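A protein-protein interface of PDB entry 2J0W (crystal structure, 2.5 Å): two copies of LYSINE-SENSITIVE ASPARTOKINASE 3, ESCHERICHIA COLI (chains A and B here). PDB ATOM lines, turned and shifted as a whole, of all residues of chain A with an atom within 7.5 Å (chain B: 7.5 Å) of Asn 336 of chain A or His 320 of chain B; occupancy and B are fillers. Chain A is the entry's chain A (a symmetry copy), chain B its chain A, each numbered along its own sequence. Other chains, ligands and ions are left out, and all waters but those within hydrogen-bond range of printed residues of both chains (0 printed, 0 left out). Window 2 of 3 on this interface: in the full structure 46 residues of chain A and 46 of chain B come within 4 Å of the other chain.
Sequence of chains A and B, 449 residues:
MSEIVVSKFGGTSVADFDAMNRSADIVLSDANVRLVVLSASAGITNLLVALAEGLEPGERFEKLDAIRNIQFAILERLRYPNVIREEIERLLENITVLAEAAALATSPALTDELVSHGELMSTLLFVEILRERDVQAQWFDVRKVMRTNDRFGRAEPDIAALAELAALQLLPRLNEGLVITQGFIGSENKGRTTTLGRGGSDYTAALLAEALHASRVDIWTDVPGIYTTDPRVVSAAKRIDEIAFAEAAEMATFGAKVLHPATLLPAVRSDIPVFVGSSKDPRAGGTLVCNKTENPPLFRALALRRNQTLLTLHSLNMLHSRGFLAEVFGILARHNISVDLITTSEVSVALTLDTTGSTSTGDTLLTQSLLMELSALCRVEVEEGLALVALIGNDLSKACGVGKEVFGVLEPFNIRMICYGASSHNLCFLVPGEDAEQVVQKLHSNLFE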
ATOM      1  N   ARG A 151     -10.201  10.632  16.539  1.00  0.00           N
ATOM      2  CA  ARG A 151     -10.282   9.361  17.261  1.00  0.00           C
ATOM      3  C   ARG A 151      -9.762   9.566  18.689  1.00  0.00           C
ATOM      4  O   ARG A 151      -8.580   9.336  18.954  1.00  0.00           O
ATOM      5  CB  ARG A 151      -9.432   8.293  16.564  1.00  0.00           C
ATOM      6  CG  ARG A 151      -9.547   6.936  17.236  1.00  0.00           C
ATOM      7  CD  ARG A 151      -8.840   5.850  16.474  1.00  0.00           C
ATOM      8  NE  ARG A 151      -9.148   4.527  17.016  1.00  0.00           N
ATOM      9  CZ  ARG A 151     -10.379   4.039  17.168  1.00  0.00           C
ATOM     10  NH1 ARG A 151     -11.438   4.762  16.828  1.00  0.00           N
ATOM     11  NH2 ARG A 151     -10.552   2.813  17.646  1.00  0.00           N
ATOM     12  N   ARG A 154      -6.826   7.637  21.440  1.00  0.00           N
ATOM     13  CA  ARG A 154      -5.655   7.189  20.710  1.00  0.00           C
ATOM     14  C   ARG A 154      -5.699   7.818  19.331  1.00  0.00           C
ATOM     15  O   ARG A 154      -5.771   7.127  18.317  1.00  0.00           O
ATOM     16  CB  ARG A 154      -5.625   5.661  20.628  1.00  0.00           C
ATOM     17  CG  ARG A 154      -6.879   5.049  20.080  1.00  0.00           C
ATOM     18  CD  ARG A 154      -6.870   3.551  20.321  1.00  0.00           C
ATOM     19  NE  ARG A 154      -7.738   2.834  19.392  1.00  0.00           N
ATOM     20  CZ  ARG A 154      -7.980   1.529  19.454  1.00  0.00           C
ATOM     21  NH1 ARG A 154      -7.423   0.790  20.411  1.00  0.00           N
ATOM     22  NH2 ARG A 154      -8.768   0.961  18.547  1.00  0.00           N
ATOM     23  N   GLU A 156      -4.694   9.728  15.918  1.00  0.00           N
ATOM     24  CA  GLU A 156      -3.616   9.451  14.988  1.00  0.00           C
ATOM     25  C   GLU A 156      -3.133  10.749  14.353  1.00  0.00           C
ATOM     26  O   GLU A 156      -3.926  11.531  13.815  1.00  0.00           O
ATOM     27  CB  GLU A 156      -4.102   8.489  13.916  1.00  0.00           C
ATOM     28  CG  GLU A 156      -4.569   7.159  14.477  1.00  0.00           C
ATOM     29  CD  GLU A 156      -5.434   6.389  13.496  1.00  0.00           C
ATOM     30  OE1 GLU A 156      -5.135   6.453  12.281  1.00  0.00           O
ATOM     31  OE2 GLU A 156      -6.397   5.718  13.938  1.00  0.00           O
ATOM     32  N   ILE A 331     -14.559  -6.505   7.543  1.00  0.00           N
ATOM     33  CA  ILE A 331     -15.484  -6.172   8.601  1.00  0.00           C
ATOM     34  C   ILE A 331     -14.639  -5.497   9.660  1.00  0.00           C
ATOM     35  O   ILE A 331     -15.058  -4.546  10.320  1.00  0.00           O
ATOM     36  CB  ILE A 331     -16.106  -7.436   9.160  1.00  0.00           C
ATOM     37  CG1 ILE A 331     -16.729  -8.212   8.006  1.00  0.00           C
ATOM     38  CG2 ILE A 331     -17.129  -7.095  10.219  1.00  0.00           C
ATOM     39  CD1 ILE A 331     -17.473  -9.439   8.429  1.00  0.00           C
ATOM     40  N   LEU A 332     -13.424  -6.007   9.799  1.00  0.00           N
ATOM     41  CA  LEU A 332     -12.477  -5.482  10.760  1.00  0.00           C
ATOM     42  C   LEU A 332     -11.960  -4.194  10.142  1.00  0.00           C
ATOM     43  O   LEU A 332     -11.357  -3.360  10.817  1.00  0.00           O
ATOM     44  CB  LEU A 332     -11.335  -6.484  10.951  1.00  0.00           C
ATOM     45  CG  LEU A 332     -11.756  -7.954  11.095  1.00  0.00           C
ATOM     46  CD1 LEU A 332     -10.532  -8.845  11.131  1.00  0.00           C
ATOM     47  CD2 LEU A 332     -12.584  -8.145  12.343  1.00  0.00           C
ATOM     48  N   ALA A 333     -12.220  -4.047   8.846  1.00  0.00           N
ATOM     49  CA  ALA A 333     -11.798  -2.872   8.091  1.00  0.00           C
ATOM     50  C   ALA A 333     -12.731  -1.709   8.370  1.00  0.00           C
ATOM     51  O   ALA A 333     -12.357  -0.546   8.224  1.00  0.00           O
ATOM     52  CB  ALA A 333     -11.798  -3.185   6.610  1.00  0.00           C
ATOM     53  N   ARG A 334     -13.957  -2.039   8.754  1.00  0.00           N
ATOM     54  CA  ARG A 334     -14.957  -1.031   9.060  1.00  0.00           C
ATOM     55  C   ARG A 334     -14.782  -0.676  10.521  1.00  0.00           C
ATOM     56  O   ARG A 334     -14.516   0.479  10.862  1.00  0.00           O
ATOM     57  CB  ARG A 334     -16.367  -1.586   8.830  1.00  0.00           C
ATOM     58  CG  ARG A 334     -16.516  -2.339   7.514  1.00  0.00           C
ATOM     59  CD  ARG A 334     -17.963  -2.698   7.176  1.00  0.00           C
ATOM     60  NE  ARG A 334     -18.027  -3.657   6.072  1.00  0.00           N
ATOM     61  CZ  ARG A 334     -17.284  -3.589   4.966  1.00  0.00           C
ATOM     62  NH1 ARG A 334     -16.403  -2.609   4.797  1.00  0.00           N
ATOM     63  NH2 ARG A 334     -17.404  -4.511   4.023  1.00  0.00           N
ATOM     64  N   HIS A 335     -14.921  -1.688  11.374  1.00  0.00           N
ATOM     65  CA  HIS A 335     -14.780  -1.516  12.815  1.00  0.00           C
ATOM     66  C   HIS A 335     -13.339  -1.147  13.143  1.00  0.00           C
ATOM     67  O   HIS A 335     -12.996  -0.899  14.297  1.00  0.00           O
ATOM     68  CB  HIS A 335     -15.132  -2.813  13.552  1.00  0.00           C
ATOM     69  CG  HIS A 335     -16.552  -3.258  13.376  1.00  0.00           C
ATOM     70  ND1 HIS A 335     -17.060  -3.674  12.165  1.00  0.00           N
ATOM     71  CD2 HIS A 335     -17.557  -3.400  14.275  1.00  0.00           C
ATOM     72  CE1 HIS A 335     -18.315  -4.057  12.325  1.00  0.00           C
ATOM     73  NE2 HIS A 335     -18.641  -3.902  13.596  1.00  0.00           N
ATOM     74  N   ASN A 336     -12.506  -1.106  12.111  1.00  0.00           N
ATOM     75  CA  ASN A 336     -11.087  -0.810  12.253  1.00  0.00           C
ATOM     76  C   ASN A 336     -10.406  -1.434  13.470  1.00  0.00           C
ATOM     77  O   ASN A 336      -9.900  -0.750  14.373  1.00  0.00           O
ATOM     78  CB  ASN A 336     -10.831   0.694  12.183  1.00  0.00           C
ATOM     79  CG  ASN A 336     -10.343   1.123  10.806  1.00  0.00           C
ATOM     80  OD1 ASN A 336     -10.072   2.298  10.562  1.00  0.00           O
ATOM     81  ND2 ASN A 336     -10.227   0.157   9.899  1.00  0.00           N
ATOM     82  N   ILE A 337     -10.418  -2.767  13.446  1.00  0.00           N
ATOM     83  CA  ILE A 337      -9.809  -3.632  14.442  1.00  0.00           C
ATOM     84  C   ILE A 337      -8.519  -4.136  13.799  1.00  0.00           C
ATOM     85  O   ILE A 337      -8.566  -4.906  12.845  1.00  0.00           O
ATOM     86  CB  ILE A 337     -10.712  -4.832  14.724  1.00  0.00           C
ATOM     87  CG1 ILE A 337     -11.984  -4.353  15.414  1.00  0.00           C
ATOM     88  CG2 ILE A 337      -9.974  -5.867  15.552  1.00  0.00           C
ATOM     89  CD1 ILE A 337     -12.949  -5.464  15.742  1.00  0.00           C
ATOM     90  N   SER A 338      -7.375  -3.694  14.299  1.00  0.00           N
ATOM     91  CA  SER A 338      -6.102  -4.112  13.738  1.00  0.00           C
ATOM     92  C   SER A 338      -5.540  -5.310  14.504  1.00  0.00           C
ATOM     93  O   SER A 338      -5.559  -5.333  15.738  1.00  0.00           O
ATOM     94  CB  SER A 338      -5.119  -2.937  13.782  1.00  0.00           C
ATOM     95  OG  SER A 338      -3.862  -3.267  13.208  1.00  0.00           O
ATOM     96  N   VAL A 339      -5.048  -6.304  13.762  1.00  0.00           N
ATOM     97  CA  VAL A 339      -4.473  -7.523  14.339  1.00  0.00           C
ATOM     98  C   VAL A 339      -3.028  -7.716  13.891  1.00  0.00           C
ATOM     99  O   VAL A 339      -2.738  -7.743  12.688  1.00  0.00           O
ATOM    100  CB  VAL A 339      -5.272  -8.772  13.914  1.00  0.00           C
ATOM    101  CG1 VAL A 339      -4.644 -10.023  14.512  1.00  0.00           C
ATOM    102  CG2 VAL A 339      -6.712  -8.628  14.357  1.00  0.00           C
ATOM    103  N   LEU A 370     -20.512  -5.617  15.830  1.00  0.00           N
ATOM    104  CA  LEU A 370     -19.520  -6.437  15.170  1.00  0.00           C
ATOM    105  C   LEU A 370     -19.880  -7.904  15.303  1.00  0.00           C
ATOM    106  O   LEU A 370     -20.098  -8.602  14.312  1.00  0.00           O
ATOM    107  CB  LEU A 370     -18.159  -6.226  15.821  1.00  0.00           C
ATOM    108  CG  LEU A 370     -17.056  -7.165  15.354  1.00  0.00           C
ATOM    109  CD1 LEU A 370     -16.761  -6.914  13.886  1.00  0.00           C
ATOM    110  CD2 LEU A 370     -15.817  -6.929  16.188  1.00  0.00           C
ATOM    111  N   ASN B 317       3.300  -0.424   1.945  1.00  0.00           N
ATOM    112  CA  ASN B 317       2.760   0.560   2.881  1.00  0.00           C
ATOM    113  C   ASN B 317       1.846   1.655   2.322  1.00  0.00           C
ATOM    114  O   ASN B 317       2.103   2.838   2.530  1.00  0.00           O
ATOM    115  CB  ASN B 317       3.964   1.169   3.635  1.00  0.00           C
ATOM    116  CG  ASN B 317       3.566   2.131   4.734  1.00  0.00           C
ATOM    117  OD1 ASN B 317       3.541   3.346   4.532  1.00  0.00           O
ATOM    118  ND2 ASN B 317       3.263   1.594   5.909  1.00  0.00           N
ATOM    119  N   MET B 318       0.770   1.284   1.631  1.00  0.00           N
ATOM    120  CA  MET B 318      -0.118   2.317   1.102  1.00  0.00           C
ATOM    121  C   MET B 318      -1.582   2.256   1.538  1.00  0.00           C
ATOM    122  O   MET B 318      -2.366   3.141   1.195  1.00  0.00           O
ATOM    123  CB  MET B 318      -0.039   2.370  -0.426  1.00  0.00           C
ATOM    124  CG  MET B 318      -0.454   1.109  -1.138  1.00  0.00           C
ATOM    125  SD  MET B 318      -0.157   1.308  -2.899  1.00  0.00           S
ATOM    126  CE  MET B 318       1.617   1.095  -2.958  1.00  0.00           C
ATOM    127  N   LEU B 319      -1.958   1.229   2.290  1.00  0.00           N
ATOM    128  CA  LEU B 319      -3.334   1.119   2.772  1.00  0.00           C
ATOM    129  C   LEU B 319      -3.284   0.684   4.237  1.00  0.00           C
ATOM    130  O   LEU B 319      -2.253   0.207   4.707  1.00  0.00           O
ATOM    131  CB  LEU B 319      -4.110   0.106   1.921  1.00  0.00           C
ATOM    132  CG  LEU B 319      -4.084   0.348   0.404  1.00  0.00           C
ATOM    133  CD1 LEU B 319      -4.623  -0.877  -0.308  1.00  0.00           C
ATOM    134  CD2 LEU B 319      -4.896   1.585   0.034  1.00  0.00           C
ATOM    135  N   HIS B 320      -4.371   0.862   4.980  1.00  0.00           N
ATOM    136  CA  HIS B 320      -4.334   0.459   6.378  1.00  0.00           C
ATOM    137  C   HIS B 320      -4.537  -1.054   6.508  1.00  0.00           C
ATOM    138  O   HIS B 320      -5.350  -1.637   5.793  1.00  0.00           O
ATOM    139  CB  HIS B 320      -5.359   1.264   7.200  1.00  0.00           C
ATOM    140  CG  HIS B 320      -6.780   1.128   6.742  1.00  0.00           C
ATOM    141  ND1 HIS B 320      -7.826   1.726   7.410  1.00  0.00           N
ATOM    142  CD2 HIS B 320      -7.337   0.428   5.724  1.00  0.00           C
ATOM    143  CE1 HIS B 320      -8.967   1.396   6.829  1.00  0.00           C
ATOM    144  NE2 HIS B 320      -8.698   0.608   5.804  1.00  0.00           N
ATOM    145  N   SER B 321      -3.769  -1.685   7.397  1.00  0.00           N
ATOM    146  CA  SER B 321      -3.834  -3.138   7.614  1.00  0.00           C
ATOM    147  C   SER B 321      -5.213  -3.735   7.358  1.00  0.00           C
ATOM    148  O   SER B 321      -5.351  -4.755   6.678  1.00  0.00           O
ATOM    149  CB  SER B 321      -3.428  -3.493   9.045  1.00  0.00           C
ATOM    150  OG  SER B 321      -4.559  -3.470   9.903  1.00  0.00           O
ATOM    151  N   ARG B 322      -6.231  -3.101   7.926  1.00  0.00           N
ATOM    152  CA  ARG B 322      -7.605  -3.560   7.772  1.00  0.00           C
ATOM    153  C   ARG B 322      -7.868  -3.863   6.307  1.00  0.00           C
ATOM    154  O   ARG B 322      -8.299  -4.960   5.961  1.00  0.00           O
ATOM    155  CB  ARG B 322      -8.573  -2.484   8.262  1.00  0.00           C
ATOM    156  CG  ARG B 322      -7.928  -1.487   9.203  1.00  0.00           C
ATOM    157  CD  ARG B 322      -7.293  -2.205  10.380  1.00  0.00           C
ATOM    158  NE  ARG B 322      -6.340  -1.369  11.105  1.00  0.00           N
ATOM    159  CZ  ARG B 322      -6.677  -0.400  11.950  1.00  0.00           C
ATOM    160  NH1 ARG B 322      -7.954  -0.132  12.186  1.00  0.00           N
ATOM    161  NH2 ARG B 322      -5.733   0.296  12.566  1.00  0.00           N
ATOM    162  N   GLY B 323      -7.598  -2.884   5.449  1.00  0.00           N
ATOM    163  CA  GLY B 323      -7.803  -3.078   4.027  1.00  0.00           C
ATOM    164  C   GLY B 323      -6.654  -3.857   3.419  1.00  0.00           C
ATOM    165  O   GLY B 323      -6.876  -4.800   2.654  1.00  0.00           O
ATOM    166  N   PHE B 324      -5.423  -3.472   3.762  1.00  0.00           N
ATOM    167  CA  PHE B 324      -4.247  -4.155   3.228  1.00  0.00           C
ATOM    168  C   PHE B 324      -4.475  -5.649   3.251  1.00  0.00           C
ATOM    169  O   PHE B 324      -3.958  -6.375   2.407  1.00  0.00           O
ATOM    170  CB  PHE B 324      -2.978  -3.855   4.029  1.00  0.00           C
ATOM    171  CG  PHE B 324      -1.788  -4.653   3.564  1.00  0.00           C
ATOM    172  CD1 PHE B 324      -1.195  -4.383   2.336  1.00  0.00           C
ATOM    173  CD2 PHE B 324      -1.309  -5.720   4.315  1.00  0.00           C
ATOM    174  CE1 PHE B 324      -0.155  -5.164   1.867  1.00  0.00           C
ATOM    175  CE2 PHE B 324      -0.266  -6.505   3.849  1.00  0.00           C
ATOM    176  CZ  PHE B 324       0.312  -6.229   2.624  1.00  0.00           C
ATOM    177  N   LEU B 325      -5.232  -6.105   4.243  1.00  0.00           N
ATOM    178  CA  LEU B 325      -5.555  -7.515   4.357  1.00  0.00           C
ATOM    179  C   LEU B 325      -6.859  -7.720   3.605  1.00  0.00           C
ATOM    180  O   LEU B 325      -6.892  -8.435   2.610  1.00  0.00           O
ATOM    181  CB  LEU B 325      -5.706  -7.928   5.827  1.00  0.00           C
ATOM    182  CG  LEU B 325      -4.450  -7.786   6.697  1.00  0.00           C
ATOM    183  CD1 LEU B 325      -4.705  -8.344   8.081  1.00  0.00           C
ATOM    184  CD2 LEU B 325      -3.296  -8.516   6.053  1.00  0.00           C
ATOM    185  N   ALA B 326      -7.923  -7.066   4.064  1.00  0.00           N
ATOM    186  CA  ALA B 326      -9.238  -7.174   3.429  1.00  0.00           C
ATOM    187  C   ALA B 326      -9.156  -7.142   1.908  1.00  0.00           C
ATOM    188  O   ALA B 326     -10.011  -7.702   1.224  1.00  0.00           O
ATOM    189  CB  ALA B 326     -10.149  -6.052   3.907  1.00  0.00           C
ATOM    190  N   GLU B 327      -8.135  -6.472   1.388  1.00  0.00           N
ATOM    191  CA  GLU B 327      -7.935  -6.367  -0.053  1.00  0.00           C
ATOM    192  C   GLU B 327      -7.186  -7.595  -0.549  1.00  0.00           C
ATOM    193  O   GLU B 327      -7.670  -8.324  -1.416  1.00  0.00           O
ATOM    194  CB  GLU B 327      -7.137  -5.104  -0.385  1.00  0.00           C
ATOM    195  CG  GLU B 327      -6.988  -4.824  -1.879  1.00  0.00           C
ATOM    196  CD  GLU B 327      -8.309  -4.908  -2.637  1.00  0.00           C
ATOM    197  OE1 GLU B 327      -9.364  -4.597  -2.044  1.00  0.00           O
ATOM    198  OE2 GLU B 327      -8.288  -5.273  -3.832  1.00  0.00           O
ATOM    199  N   VAL B 347       1.814  -6.366   9.112  1.00  0.00           N
ATOM    200  CA  VAL B 347       1.391  -6.276   7.725  1.00  0.00           C
ATOM    201  C   VAL B 347       2.137  -7.233   6.802  1.00  0.00           C
ATOM    202  O   VAL B 347       2.176  -7.039   5.584  1.00  0.00           O
ATOM    203  CB  VAL B 347       1.546  -4.831   7.202  1.00  0.00           C
ATOM    204  CG1 VAL B 347       0.381  -3.981   7.681  1.00  0.00           C
ATOM    205  CG2 VAL B 347       2.866  -4.242   7.699  1.00  0.00           C
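No position is printed for both chains. Of the 7 pairs that touch across the chains among the printed residues, none has its exchanged pair printed and touching as well.
The side-chain hydroxyl of Ser 321 of chain B lies within hydrogen-bond range of the side-chain hydroxyl of Ser 338 of chain A, 3.4 Å away. O of Asn 336 of chain A is in hydrogen-bond range of NH1 of Arg 322 of chain B, at 3.0 Å.
Printed residues of chain B that touch a printed residue of chain A: His 320, Ser 321 and Arg 322. Hydrophobic or aromatic side chains of chain B that line the printed part of chain A: His 320. Of the 13 printed residues of chain A, 5 touch a printed residue of chain B. Hydrophobic or aromatic side chains of chain A within 4 Å of the printed part of chain B: Ala 333. Among the printed residues, no Asp or Glu carboxylate lies within 4 Å of a Lys or Arg side-chain nitrogen of the other chain.
Asn 336 of chain A touches just these residues of chain B: His 320 and Arg 322. Of chain A, only Asn 336 (3.5 Å) comes within 4 Å of His 320 of chain B. Of the printed residues of chain B, Ser 338 of chain A touches Ser 321 (3.4 Å) and Arg 322 (3.3 Å). Of the printed residues of chain B, Leu 332 of chain A touches Arg 322 (3.9 Å). Printed residues of chain B within 4 Å of Ala 333 of chain A: Arg 322. Printed residues of chain B within 4 Å of Ile 337 of chain A: Arg 322 (3.8 Å). Gly 323 of chain B touches none of the printed residues of chain A. Arg 334 of chain A touches none of the printed residues of chain B. The nearest printed residue of chain B that does not touch Leu 332 of chain A is Gly 323 of chain B (6.5 Å).
The side-chain hydroxyl (OG) of Ser 321 of chain B is in hydrogen-bond range of the guanidinium group (NE) of Arg 322 of chain B (3.0 Å). The backbone carbonyl oxygen of Leu 332 of chain A lies within hydrogen-bond range of the backbone NH of Ile 337 of chain A. O of Ala 333 of chain A lies within hydrogen-bond range of ND2 of Asn 336 of chain A (2.8 Å).
Among the printed residues, merely in contact across the chains: Leu 332 of chain A with Arg 322 of chain B (3.9 Å), Ala 333 of chain A with Arg 322 of chain B (3.3 Å), Asn 336 of chain A with His 320 of chain B (3.5 Å), Ile 337 of chain A with Arg 322 of chain B (3.8 Å) and Ser 338 of chain A with Arg 322 of chain B (3.3 Å).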
